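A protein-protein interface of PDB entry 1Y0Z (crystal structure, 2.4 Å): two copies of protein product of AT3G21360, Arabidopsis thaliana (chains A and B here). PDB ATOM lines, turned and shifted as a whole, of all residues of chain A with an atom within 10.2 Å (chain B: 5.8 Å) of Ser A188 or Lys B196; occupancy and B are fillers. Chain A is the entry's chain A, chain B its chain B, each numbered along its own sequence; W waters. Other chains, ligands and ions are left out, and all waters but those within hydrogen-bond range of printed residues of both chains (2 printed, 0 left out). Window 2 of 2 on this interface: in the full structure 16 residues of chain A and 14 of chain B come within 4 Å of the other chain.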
ATOM      1  N   PRO A  97      12.284  31.414  16.839  1.00  0.00           N
ATOM      2  CA  PRO A  97      11.220  30.499  17.303  1.00  0.00           C
ATOM      3  C   PRO A  97      10.827  30.696  18.761  1.00  0.00           C
ATOM      4  O   PRO A  97      11.422  30.110  19.672  1.00  0.00           O
ATOM      5  CB  PRO A  97      11.790  29.091  17.051  1.00  0.00           C
ATOM      6  CG  PRO A  97      13.193  29.296  16.554  1.00  0.00           C
ATOM      7  CD  PRO A  97      13.234  30.693  15.977  1.00  0.00           C
ATOM      8  N   ASN A 109      14.288  29.868  22.186  1.00  0.00           N
ATOM      9  CA  ASN A 109      15.386  28.930  22.142  1.00  0.00           C
ATOM     10  C   ASN A 109      16.578  29.608  21.496  1.00  0.00           C
ATOM     11  O   ASN A 109      16.561  29.994  20.324  1.00  0.00           O
ATOM     12  CB  ASN A 109      14.973  27.671  21.382  1.00  0.00           C
ATOM     13  CG  ASN A 109      13.905  27.946  20.358  1.00  0.00           C
ATOM     14  OD1 ASN A 109      14.100  28.745  19.445  1.00  0.00           O
ATOM     15  ND2 ASN A 109      12.760  27.289  20.507  1.00  0.00           N
ATOM     16  N   GLU A 110      17.603  29.765  22.319  1.00  0.00           N
ATOM     17  CA  GLU A 110      18.849  30.391  21.944  1.00  0.00           C
ATOM     18  C   GLU A 110      19.810  29.338  21.435  1.00  0.00           C
ATOM     19  O   GLU A 110      19.458  28.165  21.302  1.00  0.00           O
ATOM     20  CB  GLU A 110      19.465  31.053  23.170  1.00  0.00           C
ATOM     21  CG  GLU A 110      18.470  31.774  24.038  1.00  0.00           C
ATOM     22  CD  GLU A 110      19.080  32.190  25.346  1.00  0.00           C
ATOM     23  OE1 GLU A 110      19.590  31.358  26.104  1.00  0.00           O
ATOM     24  OE2 GLU A 110      19.038  33.482  25.626  1.00  0.00           O
ATOM     25  N   SER A 111      21.034  29.773  21.165  1.00  0.00           N
ATOM     26  CA  SER A 111      22.074  28.874  20.710  1.00  0.00           C
ATOM     27  C   SER A 111      22.462  27.995  21.906  1.00  0.00           C
ATOM     28  O   SER A 111      22.140  28.316  23.047  1.00  0.00           O
ATOM     29  CB  SER A 111      23.272  29.689  20.220  1.00  0.00           C
ATOM     30  OG  SER A 111      23.706  30.601  21.210  1.00  0.00           O
ATOM     31  N   PRO A 112      23.144  26.865  21.655  1.00  0.00           N
ATOM     32  CA  PRO A 112      23.585  25.924  22.695  1.00  0.00           C
ATOM     33  C   PRO A 112      24.281  26.601  23.874  1.00  0.00           C
ATOM     34  O   PRO A 112      24.826  27.690  23.731  1.00  0.00           O
ATOM     35  CB  PRO A 112      24.520  24.996  21.929  1.00  0.00           C
ATOM     36  CG  PRO A 112      23.877  24.935  20.586  1.00  0.00           C
ATOM     37  CD  PRO A 112      23.531  26.378  20.318  1.00  0.00           C
ATOM     38  N   PRO A 113      24.260  25.962  25.058  1.00  0.00           N
ATOM     39  CA  PRO A 113      24.883  26.481  26.284  1.00  0.00           C
ATOM     40  C   PRO A 113      26.379  26.777  26.223  1.00  0.00           C
ATOM     41  O   PRO A 113      26.865  27.666  26.921  1.00  0.00           O
ATOM     42  CB  PRO A 113      24.551  25.412  27.326  1.00  0.00           C
ATOM     43  CG  PRO A 113      24.293  24.195  26.518  1.00  0.00           C
ATOM     44  CD  PRO A 113      23.528  24.721  25.347  1.00  0.00           C
ATOM     45  N   ASP A 114      27.107  26.037  25.393  1.00  0.00           N
ATOM     46  CA  ASP A 114      28.547  26.232  25.275  1.00  0.00           C
ATOM     47  C   ASP A 114      28.913  27.503  24.507  1.00  0.00           C
ATOM     48  O   ASP A 114      30.047  27.977  24.576  1.00  0.00           O
ATOM     49  CB  ASP A 114      29.180  25.024  24.589  1.00  0.00           C
ATOM     50  CG  ASP A 114      28.774  24.905  23.133  1.00  0.00           C
ATOM     51  OD1 ASP A 114      27.559  24.897  22.845  1.00  0.00           O
ATOM     52  OD2 ASP A 114      29.669  24.814  22.273  1.00  0.00           O
ATOM     53  N   GLN A 115      27.958  28.061  23.777  1.00  0.00           N
ATOM     54  CA  GLN A 115      28.237  29.261  23.010  1.00  0.00           C
ATOM     55  C   GLN A 115      28.095  30.578  23.760  1.00  0.00           C
ATOM     56  O   GLN A 115      27.501  30.653  24.839  1.00  0.00           O
ATOM     57  CB  GLN A 115      27.381  29.275  21.746  1.00  0.00           C
ATOM     58  CG  GLN A 115      27.990  28.432  20.640  1.00  0.00           C
ATOM     59  CD  GLN A 115      27.083  28.263  19.437  1.00  0.00           C
ATOM     60  OE1 GLN A 115      26.527  29.231  18.920  1.00  0.00           O
ATOM     61  NE2 GLN A 115      26.942  27.025  18.977  1.00  0.00           N
ATOM     62  N   LYS A 116      28.662  31.615  23.160  1.00  0.00           N
ATOM     63  CA  LYS A 116      28.653  32.969  23.698  1.00  0.00           C
ATOM     64  C   LYS A 116      27.741  33.785  22.770  1.00  0.00           C
ATOM     65  O   LYS A 116      27.999  33.877  21.570  1.00  0.00           O
ATOM     66  CB  LYS A 116      30.079  33.522  23.638  1.00  0.00           C
ATOM     67  CG  LYS A 116      30.471  34.579  24.652  1.00  0.00           C
ATOM     68  CD  LYS A 116      31.821  35.194  24.238  1.00  0.00           C
ATOM     69  CE  LYS A 116      32.855  35.243  25.367  1.00  0.00           C
ATOM     70  NZ  LYS A 116      34.141  35.875  24.910  1.00  0.00           N
ATOM     71  N   ASP A 184      14.444  25.587   7.218  1.00  0.00           N
ATOM     72  CA  ASP A 184      14.094  25.199   8.573  1.00  0.00           C
ATOM     73  C   ASP A 184      14.993  25.903   9.582  1.00  0.00           C
ATOM     74  O   ASP A 184      15.853  26.696   9.203  1.00  0.00           O
ATOM     75  CB  ASP A 184      14.206  23.683   8.712  1.00  0.00           C
ATOM     76  CG  ASP A 184      13.436  22.951   7.631  1.00  0.00           C
ATOM     77  OD1 ASP A 184      12.248  23.280   7.429  1.00  0.00           O
ATOM     78  OD2 ASP A 184      14.017  22.056   6.980  1.00  0.00           O
ATOM     79  N   ASP A 185      14.792  25.622  10.865  1.00  0.00           N
ATOM     80  CA  ASP A 185      15.593  26.252  11.906  1.00  0.00           C
ATOM     81  C   ASP A 185      16.706  25.326  12.381  1.00  0.00           C
ATOM     82  O   ASP A 185      16.452  24.181  12.751  1.00  0.00           O
ATOM     83  CB  ASP A 185      14.706  26.640  13.090  1.00  0.00           C
ATOM     84  CG  ASP A 185      13.457  27.391  12.662  1.00  0.00           C
ATOM     85  OD1 ASP A 185      13.568  28.335  11.852  1.00  0.00           O
ATOM     86  OD2 ASP A 185      12.360  27.042  13.145  1.00  0.00           O
ATOM     87  N   ASP A 186      17.938  25.825  12.362  1.00  0.00           N
ATOM     88  CA  ASP A 186      19.090  25.044  12.796  1.00  0.00           C
ATOM     89  C   ASP A 186      19.270  25.273  14.289  1.00  0.00           C
ATOM     90  O   ASP A 186      19.670  26.354  14.716  1.00  0.00           O
ATOM     91  CB  ASP A 186      20.353  25.490  12.060  1.00  0.00           C
ATOM     92  CG  ASP A 186      21.529  24.563  12.306  1.00  0.00           C
ATOM     93  OD1 ASP A 186      21.681  24.067  13.442  1.00  0.00           O
ATOM     94  OD2 ASP A 186      22.310  24.337  11.362  1.00  0.00           O
ATOM     95  N   PRO A 187      18.984  24.250  15.103  1.00  0.00           N
ATOM     96  CA  PRO A 187      19.118  24.369  16.556  1.00  0.00           C
ATOM     97  C   PRO A 187      20.564  24.546  16.980  1.00  0.00           C
ATOM     98  O   PRO A 187      20.847  25.101  18.044  1.00  0.00           O
ATOM     99  CB  PRO A 187      18.531  23.058  17.055  1.00  0.00           C
ATOM    100  CG  PRO A 187      18.961  22.100  15.989  1.00  0.00           C
ATOM    101  CD  PRO A 187      18.655  22.865  14.719  1.00  0.00           C
ATOM    102  N   SER A 188      21.469  24.073  16.132  1.00  0.00           N
ATOM    103  CA  SER A 188      22.898  24.141  16.395  1.00  0.00           C
ATOM    104  C   SER A 188      23.575  25.458  15.982  1.00  0.00           C
ATOM    105  O   SER A 188      24.750  25.668  16.279  1.00  0.00           O
ATOM    106  CB  SER A 188      23.590  22.965  15.696  1.00  0.00           C
ATOM    107  OG  SER A 188      24.990  22.985  15.905  1.00  0.00           O
ATOM    108  N   SER A 189      22.846  26.348  15.318  1.00  0.00           N
ATOM    109  CA  SER A 189      23.443  27.605  14.878  1.00  0.00           C
ATOM    110  C   SER A 189      23.146  28.826  15.746  1.00  0.00           C
ATOM    111  O   SER A 189      22.089  28.917  16.372  1.00  0.00           O
ATOM    112  CB  SER A 189      23.012  27.908  13.441  1.00  0.00           C
ATOM    113  OG  SER A 189      23.482  29.179  13.030  1.00  0.00           O
ATOM    114  N   PRO A 190      24.092  29.783  15.795  1.00  0.00           N
ATOM    115  CA  PRO A 190      23.943  31.016  16.576  1.00  0.00           C
ATOM    116  C   PRO A 190      22.836  31.865  15.975  1.00  0.00           C
ATOM    117  O   PRO A 190      22.234  32.696  16.652  1.00  0.00           O
ATOM    118  CB  PRO A 190      25.291  31.700  16.407  1.00  0.00           C
ATOM    119  CG  PRO A 190      26.226  30.569  16.234  1.00  0.00           C
ATOM    120  CD  PRO A 190      25.472  29.658  15.296  1.00  0.00           C
ATOM    121  N   ILE A 191      22.601  31.651  14.686  1.00  0.00           N
ATOM    122  CA  ILE A 191      21.597  32.381  13.934  1.00  0.00           C
ATOM    123  C   ILE A 191      20.860  31.353  13.107  1.00  0.00           C
ATOM    124  O   ILE A 191      20.744  31.482  11.889  1.00  0.00           O
ATOM    125  CB  ILE A 191      22.277  33.399  13.005  1.00  0.00           C
ATOM    126  CG1 ILE A 191      23.374  32.699  12.181  1.00  0.00           C
ATOM    127  CG2 ILE A 191      22.843  34.535  13.826  1.00  0.00           C
ATOM    128  CD1 ILE A 191      24.077  33.596  11.202  1.00  0.00           C
ATOM    129  N   GLY A 192      20.353  30.333  13.794  1.00  0.00           N
ATOM    130  CA  GLY A 192      19.668  29.236  13.131  1.00  0.00           C
ATOM    131  C   GLY A 192      18.234  29.367  12.649  1.00  0.00           C
ATOM    132  O   GLY A 192      17.725  28.427  12.043  1.00  0.00           O
ATOM    133  N   ARG A 193      17.567  30.490  12.886  1.00  0.00           N
ATOM    134  CA  ARG A 193      16.185  30.602  12.430  1.00  0.00           C
ATOM    135  C   ARG A 193      16.126  30.585  10.911  1.00  0.00           C
ATOM    136  O   ARG A 193      16.934  31.227  10.246  1.00  0.00           O
ATOM    137  CB  ARG A 193      15.543  31.872  12.968  1.00  0.00           C
ATOM    138  CG  ARG A 193      16.378  33.097  12.781  1.00  0.00           C
ATOM    139  CD  ARG A 193      15.905  34.185  13.709  1.00  0.00           C
ATOM    140  NE  ARG A 193      15.229  35.240  12.977  1.00  0.00           N
ATOM    141  CZ  ARG A 193      15.807  35.944  12.018  1.00  0.00           C
ATOM    142  NH1 ARG A 193      17.064  35.699  11.683  1.00  0.00           N
ATOM    143  NH2 ARG A 193      15.137  36.900  11.401  1.00  0.00           N
ATOM    144  N   GLY A 257      29.515  36.975  15.134  1.00  0.00           N
ATOM    145  CA  GLY A 257      28.606  35.885  15.445  1.00  0.00           C
ATOM    146  C   GLY A 257      27.709  35.287  14.380  1.00  0.00           C
ATOM    147  O   GLY A 257      27.123  34.238  14.615  1.00  0.00           O
ATOM    148  N   GLU A 259      27.924  33.323  12.083  1.00  0.00           N
ATOM    149  CA  GLU A 259      28.748  32.268  11.525  1.00  0.00           C
ATOM    150  C   GLU A 259      28.126  30.879  11.562  1.00  0.00           C
ATOM    151  O   GLU A 259      27.865  30.330  12.631  1.00  0.00           O
ATOM    152  CB  GLU A 259      30.083  32.219  12.266  1.00  0.00           C
ATOM    153  CG  GLU A 259      31.096  31.276  11.652  1.00  0.00           C
ATOM    154  CD  GLU A 259      32.295  31.050  12.549  1.00  0.00           C
ATOM    155  OE1 GLU A 259      32.818  32.035  13.111  1.00  0.00           O
ATOM    156  OE2 GLU A 259      32.719  29.885  12.691  1.00  0.00           O
ATOM    157  N   ASP A 260      27.893  30.326  10.377  1.00  0.00           N
ATOM    158  CA  ASP A 260      27.367  28.979  10.221  1.00  0.00           C
ATOM    159  C   ASP A 260      27.650  28.525   8.788  1.00  0.00           C
ATOM    160  O   ASP A 260      28.305  29.239   8.029  1.00  0.00           O
ATOM    161  CB  ASP A 260      25.860  28.904  10.546  1.00  0.00           C
ATOM    162  CG  ASP A 260      24.986  29.660   9.561  1.00  0.00           C
ATOM    163  OD1 ASP A 260      25.350  29.780   8.373  1.00  0.00           O
ATOM    164  OD2 ASP A 260      23.900  30.117   9.980  1.00  0.00           O
ATOM    165  N   LYS A 261      27.156  27.345   8.428  1.00  0.00           N
ATOM    166  CA  LYS A 261      27.355  26.779   7.095  1.00  0.00           C
ATOM    167  C   LYS A 261      26.979  27.678   5.921  1.00  0.00           C
ATOM    168  O   LYS A 261      27.449  27.472   4.800  1.00  0.00           O
ATOM    169  CB  LYS A 261      26.544  25.498   6.952  1.00  0.00           C
ATOM    170  CG  LYS A 261      27.226  24.264   7.440  1.00  0.00           C
ATOM    171  CD  LYS A 261      26.567  23.055   6.817  1.00  0.00           C
ATOM    172  CE  LYS A 261      27.478  21.850   6.901  1.00  0.00           C
ATOM    173  NZ  LYS A 261      26.976  20.714   6.082  1.00  0.00           N
ATOM    174  N   ARG A 262      26.117  28.655   6.181  1.00  0.00           N
ATOM    175  CA  ARG A 262      25.618  29.559   5.149  1.00  0.00           C
ATOM    176  C   ARG A 262      26.105  30.989   5.286  1.00  0.00           C
ATOM    177  O   ARG A 262      25.880  31.814   4.398  1.00  0.00           O
ATOM    178  CB  ARG A 262      24.090  29.577   5.187  1.00  0.00           C
ATOM    179  CG  ARG A 262      23.451  28.210   5.069  1.00  0.00           C
ATOM    180  CD  ARG A 262      21.967  28.238   5.406  1.00  0.00           C
ATOM    181  NE  ARG A 262      21.650  27.232   6.415  1.00  0.00           N
ATOM    182  CZ  ARG A 262      21.636  27.457   7.727  1.00  0.00           C
ATOM    183  NH1 ARG A 262      21.880  28.669   8.205  1.00  0.00           N
ATOM    184  NH2 ARG A 262      21.347  26.472   8.562  1.00  0.00           N
ATOM    185  N   ARG A 315      24.788  36.822  26.447  1.00  0.00           N
ATOM    186  CA  ARG A 315      24.684  35.636  27.266  1.00  0.00           C
ATOM    187  C   ARG A 315      26.017  34.896  27.259  1.00  0.00           C
ATOM    188  O   ARG A 315      26.652  34.714  26.214  1.00  0.00           O
ATOM    189  CB  ARG A 315      23.552  34.738  26.766  1.00  0.00           C
ATOM    190  CG  ARG A 315      23.216  33.606  27.715  1.00  0.00           C
ATOM    191  CD  ARG A 315      23.814  32.308  27.228  1.00  0.00           C
ATOM    192  NE  ARG A 315      22.947  31.676  26.247  1.00  0.00           N
ATOM    193  CZ  ARG A 315      23.322  30.702  25.428  1.00  0.00           C
ATOM    194  NH1 ARG A 315      24.564  30.248  25.452  1.00  0.00           N
ATOM    195  NH2 ARG A 315      22.452  30.190  24.574  1.00  0.00           N
ATOM    196  N   GLY B 182      14.643  15.235   9.455  1.00  0.00           N
ATOM    197  CA  GLY B 182      15.555  16.089   8.722  1.00  0.00           C
ATOM    198  C   GLY B 182      16.664  16.351   9.719  1.00  0.00           C
ATOM    199  O   GLY B 182      16.569  15.888  10.856  1.00  0.00           O
ATOM    200  N   GLU B 183      17.698  17.091   9.332  1.00  0.00           N
ATOM    201  CA  GLU B 183      18.772  17.398  10.265  1.00  0.00           C
ATOM    202  C   GLU B 183      18.344  18.522  11.187  1.00  0.00           C
ATOM    203  O   GLU B 183      18.632  18.504  12.387  1.00  0.00           O
ATOM    204  CB  GLU B 183      20.060  17.780   9.525  1.00  0.00           C
ATOM    205  CG  GLU B 183      21.248  18.038  10.458  1.00  0.00           C
ATOM    206  CD  GLU B 183      22.380  18.823   9.804  1.00  0.00           C
ATOM    207  OE1 GLU B 183      22.393  18.951   8.565  1.00  0.00           O
ATOM    208  OE2 GLU B 183      23.269  19.306  10.538  1.00  0.00           O
ATOM    209  N   ASP B 184      17.641  19.500  10.623  1.00  0.00           N
ATOM    210  CA  ASP B 184      17.156  20.626  11.413  1.00  0.00           C
ATOM    211  C   ASP B 184      15.659  20.517  11.644  1.00  0.00           C
ATOM    212  O   ASP B 184      14.980  19.619  11.129  1.00  0.00           O
ATOM    213  CB  ASP B 184      17.485  21.975  10.749  1.00  0.00           C
ATOM    214  CG  ASP B 184      18.994  22.215  10.591  1.00  0.00           C
ATOM    215  OD1 ASP B 184      19.699  22.335  11.618  1.00  0.00           O
ATOM    216  OD2 ASP B 184      19.463  22.294   9.436  1.00  0.00           O
ATOM    217  N   ASP B 185      15.144  21.477  12.390  1.00  0.00           N
ATOM    218  CA  ASP B 185      13.744  21.477  12.747  1.00  0.00           C
ATOM    219  C   ASP B 185      12.851  22.258  11.785  1.00  0.00           C
ATOM    220  O   ASP B 185      13.079  23.438  11.527  1.00  0.00           O
ATOM    221  CB  ASP B 185      13.594  22.032  14.165  1.00  0.00           C
ATOM    222  CG  ASP B 185      14.533  21.349  15.178  1.00  0.00           C
ATOM    223  OD1 ASP B 185      14.606  20.097  15.220  1.00  0.00           O
ATOM    224  OD2 ASP B 185      15.196  22.069  15.943  1.00  0.00           O
ATOM    225  N   GLY B 194      13.843  17.784  13.961  1.00  0.00           N
ATOM    226  CA  GLY B 194      14.972  17.049  13.394  1.00  0.00           C
ATOM    227  C   GLY B 194      15.723  16.180  14.393  1.00  0.00           C
ATOM    228  O   GLY B 194      15.486  16.275  15.602  1.00  0.00           O
ATOM    229  N   TRP B 195      16.647  15.357  13.893  1.00  0.00           N
ATOM    230  CA  TRP B 195      17.416  14.455  14.742  1.00  0.00           C
ATOM    231  C   TRP B 195      18.369  15.161  15.696  1.00  0.00           C
ATOM    232  O   TRP B 195      18.684  14.635  16.764  1.00  0.00           O
ATOM    233  CB  TRP B 195      18.172  13.419  13.891  1.00  0.00           C
ATOM    234  CG  TRP B 195      19.299  13.929  13.027  1.00  0.00           C
ATOM    235  CD1 TRP B 195      19.261  14.175  11.680  1.00  0.00           C
ATOM    236  CD2 TRP B 195      20.654  14.152  13.435  1.00  0.00           C
ATOM    237  NE1 TRP B 195      20.511  14.528  11.226  1.00  0.00           N
ATOM    238  CE2 TRP B 195      21.384  14.524  12.282  1.00  0.00           C
ATOM    239  CE3 TRP B 195      21.323  14.072  14.664  1.00  0.00           C
ATOM    240  CZ2 TRP B 195      22.753  14.815  12.321  1.00  0.00           C
ATOM    241  CZ3 TRP B 195      22.686  14.362  14.705  1.00  0.00           C
ATOM    242  CH2 TRP B 195      23.385  14.729  13.537  1.00  0.00           C
ATOM    243  N   LYS B 196      18.820  16.354  15.325  1.00  0.00           N
ATOM    244  CA  LYS B 196      19.714  17.095  16.202  1.00  0.00           C
ATOM    245  C   LYS B 196      18.974  17.411  17.495  1.00  0.00           C
ATOM    246  O   LYS B 196      19.476  17.150  18.589  1.00  0.00           O
ATOM    247  CB  LYS B 196      20.166  18.409  15.565  1.00  0.00           C
ATOM    248  CG  LYS B 196      21.166  18.282  14.432  1.00  0.00           C
ATOM    249  CD  LYS B 196      22.401  19.146  14.688  1.00  0.00           C
ATOM    250  CE  LYS B 196      22.938  19.746  13.399  1.00  0.00           C
ATOM    251  NZ  LYS B 196      21.970  20.725  12.808  1.00  0.00           N
ATOM    252  N   SER B 197      17.778  17.975  17.352  1.00  0.00           N
ATOM    253  CA  SER B 197      16.946  18.353  18.489  1.00  0.00           C
ATOM    254  C   SER B 197      16.312  17.143  19.167  1.00  0.00           C
ATOM    255  O   SER B 197      16.209  17.095  20.391  1.00  0.00           O
ATOM    256  CB  SER B 197      15.850  19.319  18.030  1.00  0.00           C
ATOM    257  OG  SER B 197      16.403  20.529  17.539  1.00  0.00           O
ATOM    258  N   THR B 198      15.893  16.169  18.365  1.00  0.00           N
ATOM    259  CA  THR B 198      15.264  14.967  18.895  1.00  0.00           C
ATOM    260  C   THR B 198      16.205  14.189  19.799  1.00  0.00           C
ATOM    261  O   THR B 198      15.803  13.713  20.863  1.00  0.00           O
ATOM    262  CB  THR B 198      14.804  14.035  17.769  1.00  0.00           C
ATOM    263  OG1 THR B 198      13.822  14.703  16.972  1.00  0.00           O
ATOM    264  CG2 THR B 198      14.196  12.766  18.344  1.00  0.00           C
ATOM    265  N   PHE B 199      17.456  14.064  19.373  1.00  0.00           N
ATOM    266  CA  PHE B 199      18.455  13.330  20.138  1.00  0.00           C
ATOM    267  C   PHE B 199      19.443  14.258  20.847  1.00  0.00           C
ATOM    268  O   PHE B 199      20.493  13.820  21.325  1.00  0.00           O
ATOM    269  CB  PHE B 199      19.194  12.370  19.210  1.00  0.00           C
ATOM    270  CG  PHE B 199      18.293  11.395  18.514  1.00  0.00           C
ATOM    271  CD1 PHE B 199      17.638  10.400  19.229  1.00  0.00           C
ATOM    272  CD2 PHE B 199      18.083  11.480  17.145  1.00  0.00           C
ATOM    273  CE1 PHE B 199      16.785   9.500  18.588  1.00  0.00           C
ATOM    274  CE2 PHE B 199      17.232  10.585  16.496  1.00  0.00           C
ATOM    275  CZ  PHE B 199      16.582   9.595  17.221  1.00  0.00           C
ATOM    276  N   LEU B 200      19.095  15.541  20.899  1.00  0.00           N
ATOM    277  CA  LEU B 200      19.911  16.556  21.565  1.00  0.00           C
ATOM    278  C   LEU B 200      21.404  16.498  21.249  1.00  0.00           C
ATOM    279  O   LEU B 200      22.237  16.614  22.151  1.00  0.00           O
ATOM    280  CB  LEU B 200      19.710  16.457  23.081  1.00  0.00           C
ATOM    281  CG  LEU B 200      18.273  16.653  23.571  1.00  0.00           C
ATOM    282  CD1 LEU B 200      18.198  16.394  25.064  1.00  0.00           C
ATOM    283  CD2 LEU B 200      17.808  18.066  23.241  1.00  0.00           C
ATOM    284  N   THR B 201      21.743  16.330  19.973  1.00  0.00           N
ATOM    285  CA  THR B 201      23.147  16.265  19.571  1.00  0.00           C
ATOM    286  C   THR B 201      23.318  16.478  18.074  1.00  0.00           C
ATOM    287  O   THR B 201      22.399  16.241  17.292  1.00  0.00           O
ATOM    288  CB  THR B 201      23.775  14.896  19.914  1.00  0.00           C
ATOM    289  OG1 THR B 201      23.415  14.520  21.249  1.00  0.00           O
ATOM    290  CG2 THR B 201      25.298  14.971  19.811  1.00  0.00           C
ATOM    291  N   HIS B 202      24.504  16.927  17.682  1.00  0.00           N
ATOM    292  CA  HIS B 202      24.809  17.140  16.274  1.00  0.00           C
ATOM    293  C   HIS B 202      25.753  16.023  15.834  1.00  0.00           C
ATOM    294  O   HIS B 202      26.067  15.884  14.651  1.00  0.00           O
ATOM    295  CB  HIS B 202      25.472  18.506  16.063  1.00  0.00           C
ATOM    296  CG  HIS B 202      26.771  18.666  16.789  1.00  0.00           C
ATOM    297  ND1 HIS B 202      26.866  18.619  18.163  1.00  0.00           N
ATOM    298  CD2 HIS B 202      28.029  18.859  16.330  1.00  0.00           C
ATOM    299  CE1 HIS B 202      28.128  18.776  18.520  1.00  0.00           C
ATOM    300  NE2 HIS B 202      28.854  18.924  17.427  1.00  0.00           N
HETATM  301  O   HOH W   1      25.580  19.182   7.537  1.00  0.00           O
HETATM  302  O   HOH W   2      22.561  22.778   9.200  1.00  0.00           O
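OD1 of Asp A186 sits close to OD1 of Asp B184 (3.2 Å).
O of Asp B185 sits at hydrogen-bond distance from N of Asp A185.
OD1 of Asp A186 is in salt-bridge range of NZ of Lys B196.
OD2 of Asp B185 lies within hydrogen-bond range of OG of Ser B197, 2.5 Å away.
The side-chain carboxylate (OE2) of Glu B183 is in salt-bridge range of the side-chain amino group (NZ) of Lys B196.
OD1 of Asp A186 lies within hydrogen-bond range of N of Ser A189.
The side-chain carboxylate of Asp A186 lies within hydrogen-bond range of the backbone NH of Ser A188 (2.7 Å).
The side-chain carboxylate of Asp B184 is in salt-bridge range of the side-chain amino group of Lys B196 (3.0 Å).
N of Gly B194 lies within hydrogen-bond range of OD1 of Asp B185.
Among the printed residues, pairs that only touch across the chains: Asp A184 with Asp B185 (3.0 Å), Asp A185 with Asp B184 (3.2 Å), Pro A187 with Asp B184 (3.3 Å), Pro A187 with Ser B197 (3.3 Å), Pro A187 with Asp B185 (3.7 Å), Pro A187 with Lys B196 (3.9 Å) and Ser A188 with Lys B196 (3.998 Å).
Of the printed residues of chain B, Asp A184 touches Asp B185 (3.0 Å).
Of the printed residues of chain B, Asp A186 touches Asp B184 and Lys B196.
Printed residues of chain B within 4 Å of Pro A187: Asp B184 (3.3 Å), Asp B185 (3.7 Å), Lys B196 (3.9 Å) and Ser B197 (3.3 Å).
Of the printed residues of chain B, Ser A188 touches Lys B196 (3.998 Å).
No residue of chain A comes within 4 Å of Glu B183.
Of the printed residues of chain A, Asp B184 touches Asp A185, Asp A186 and Pro A187.
Of the printed residues of chain A, Asp B185 touches Asp A184 (3.0 Å), Asp A185 (2.9 Å) and Pro A187 (3.7 Å).
Printed residues of chain A within 4 Å of Lys B196: Asp A186, Pro A187 and Ser A188.
Printed residues of chain A within 4 Å of Ser B197: Pro A187 (3.3 Å).
Of the 13 printed residues of chain B, 4 touch a printed residue of chain A.
Of the 25 printed residues of chain A, 5 touch a printed residue of chain B.
Hydrophobic or aromatic side chains of chain A that line the printed part of chain B: Pro A187.
Among the printed residues, Asp or Glu carboxylates within 4 Å of a Lys or Arg side-chain nitrogen of the other chain: Asp A186 with Lys B196 (3.4 Å).
Asp A184 touches Asp B185, and with the chains exchanged Asp A185 touches Asp B184.
Asp A185 touches its own counterpart, Asp B185.
Positions printed for both chains: 184 and 185.
Of the 10 pairs that touch across the chains among the printed residues, 3 have their exchanged pair printed and touching as well.
Water W1 lies within hydrogen-bond range of NZ of Lys A261 (2.5 Å) and OE1 of Glu B183 (3.4 Å).
Water W2 lies within hydrogen-bond range of the side-chain carboxylate of Asp A186 (2.7 Å) and the side-chain carboxylate of Asp B184 (3.1 Å).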
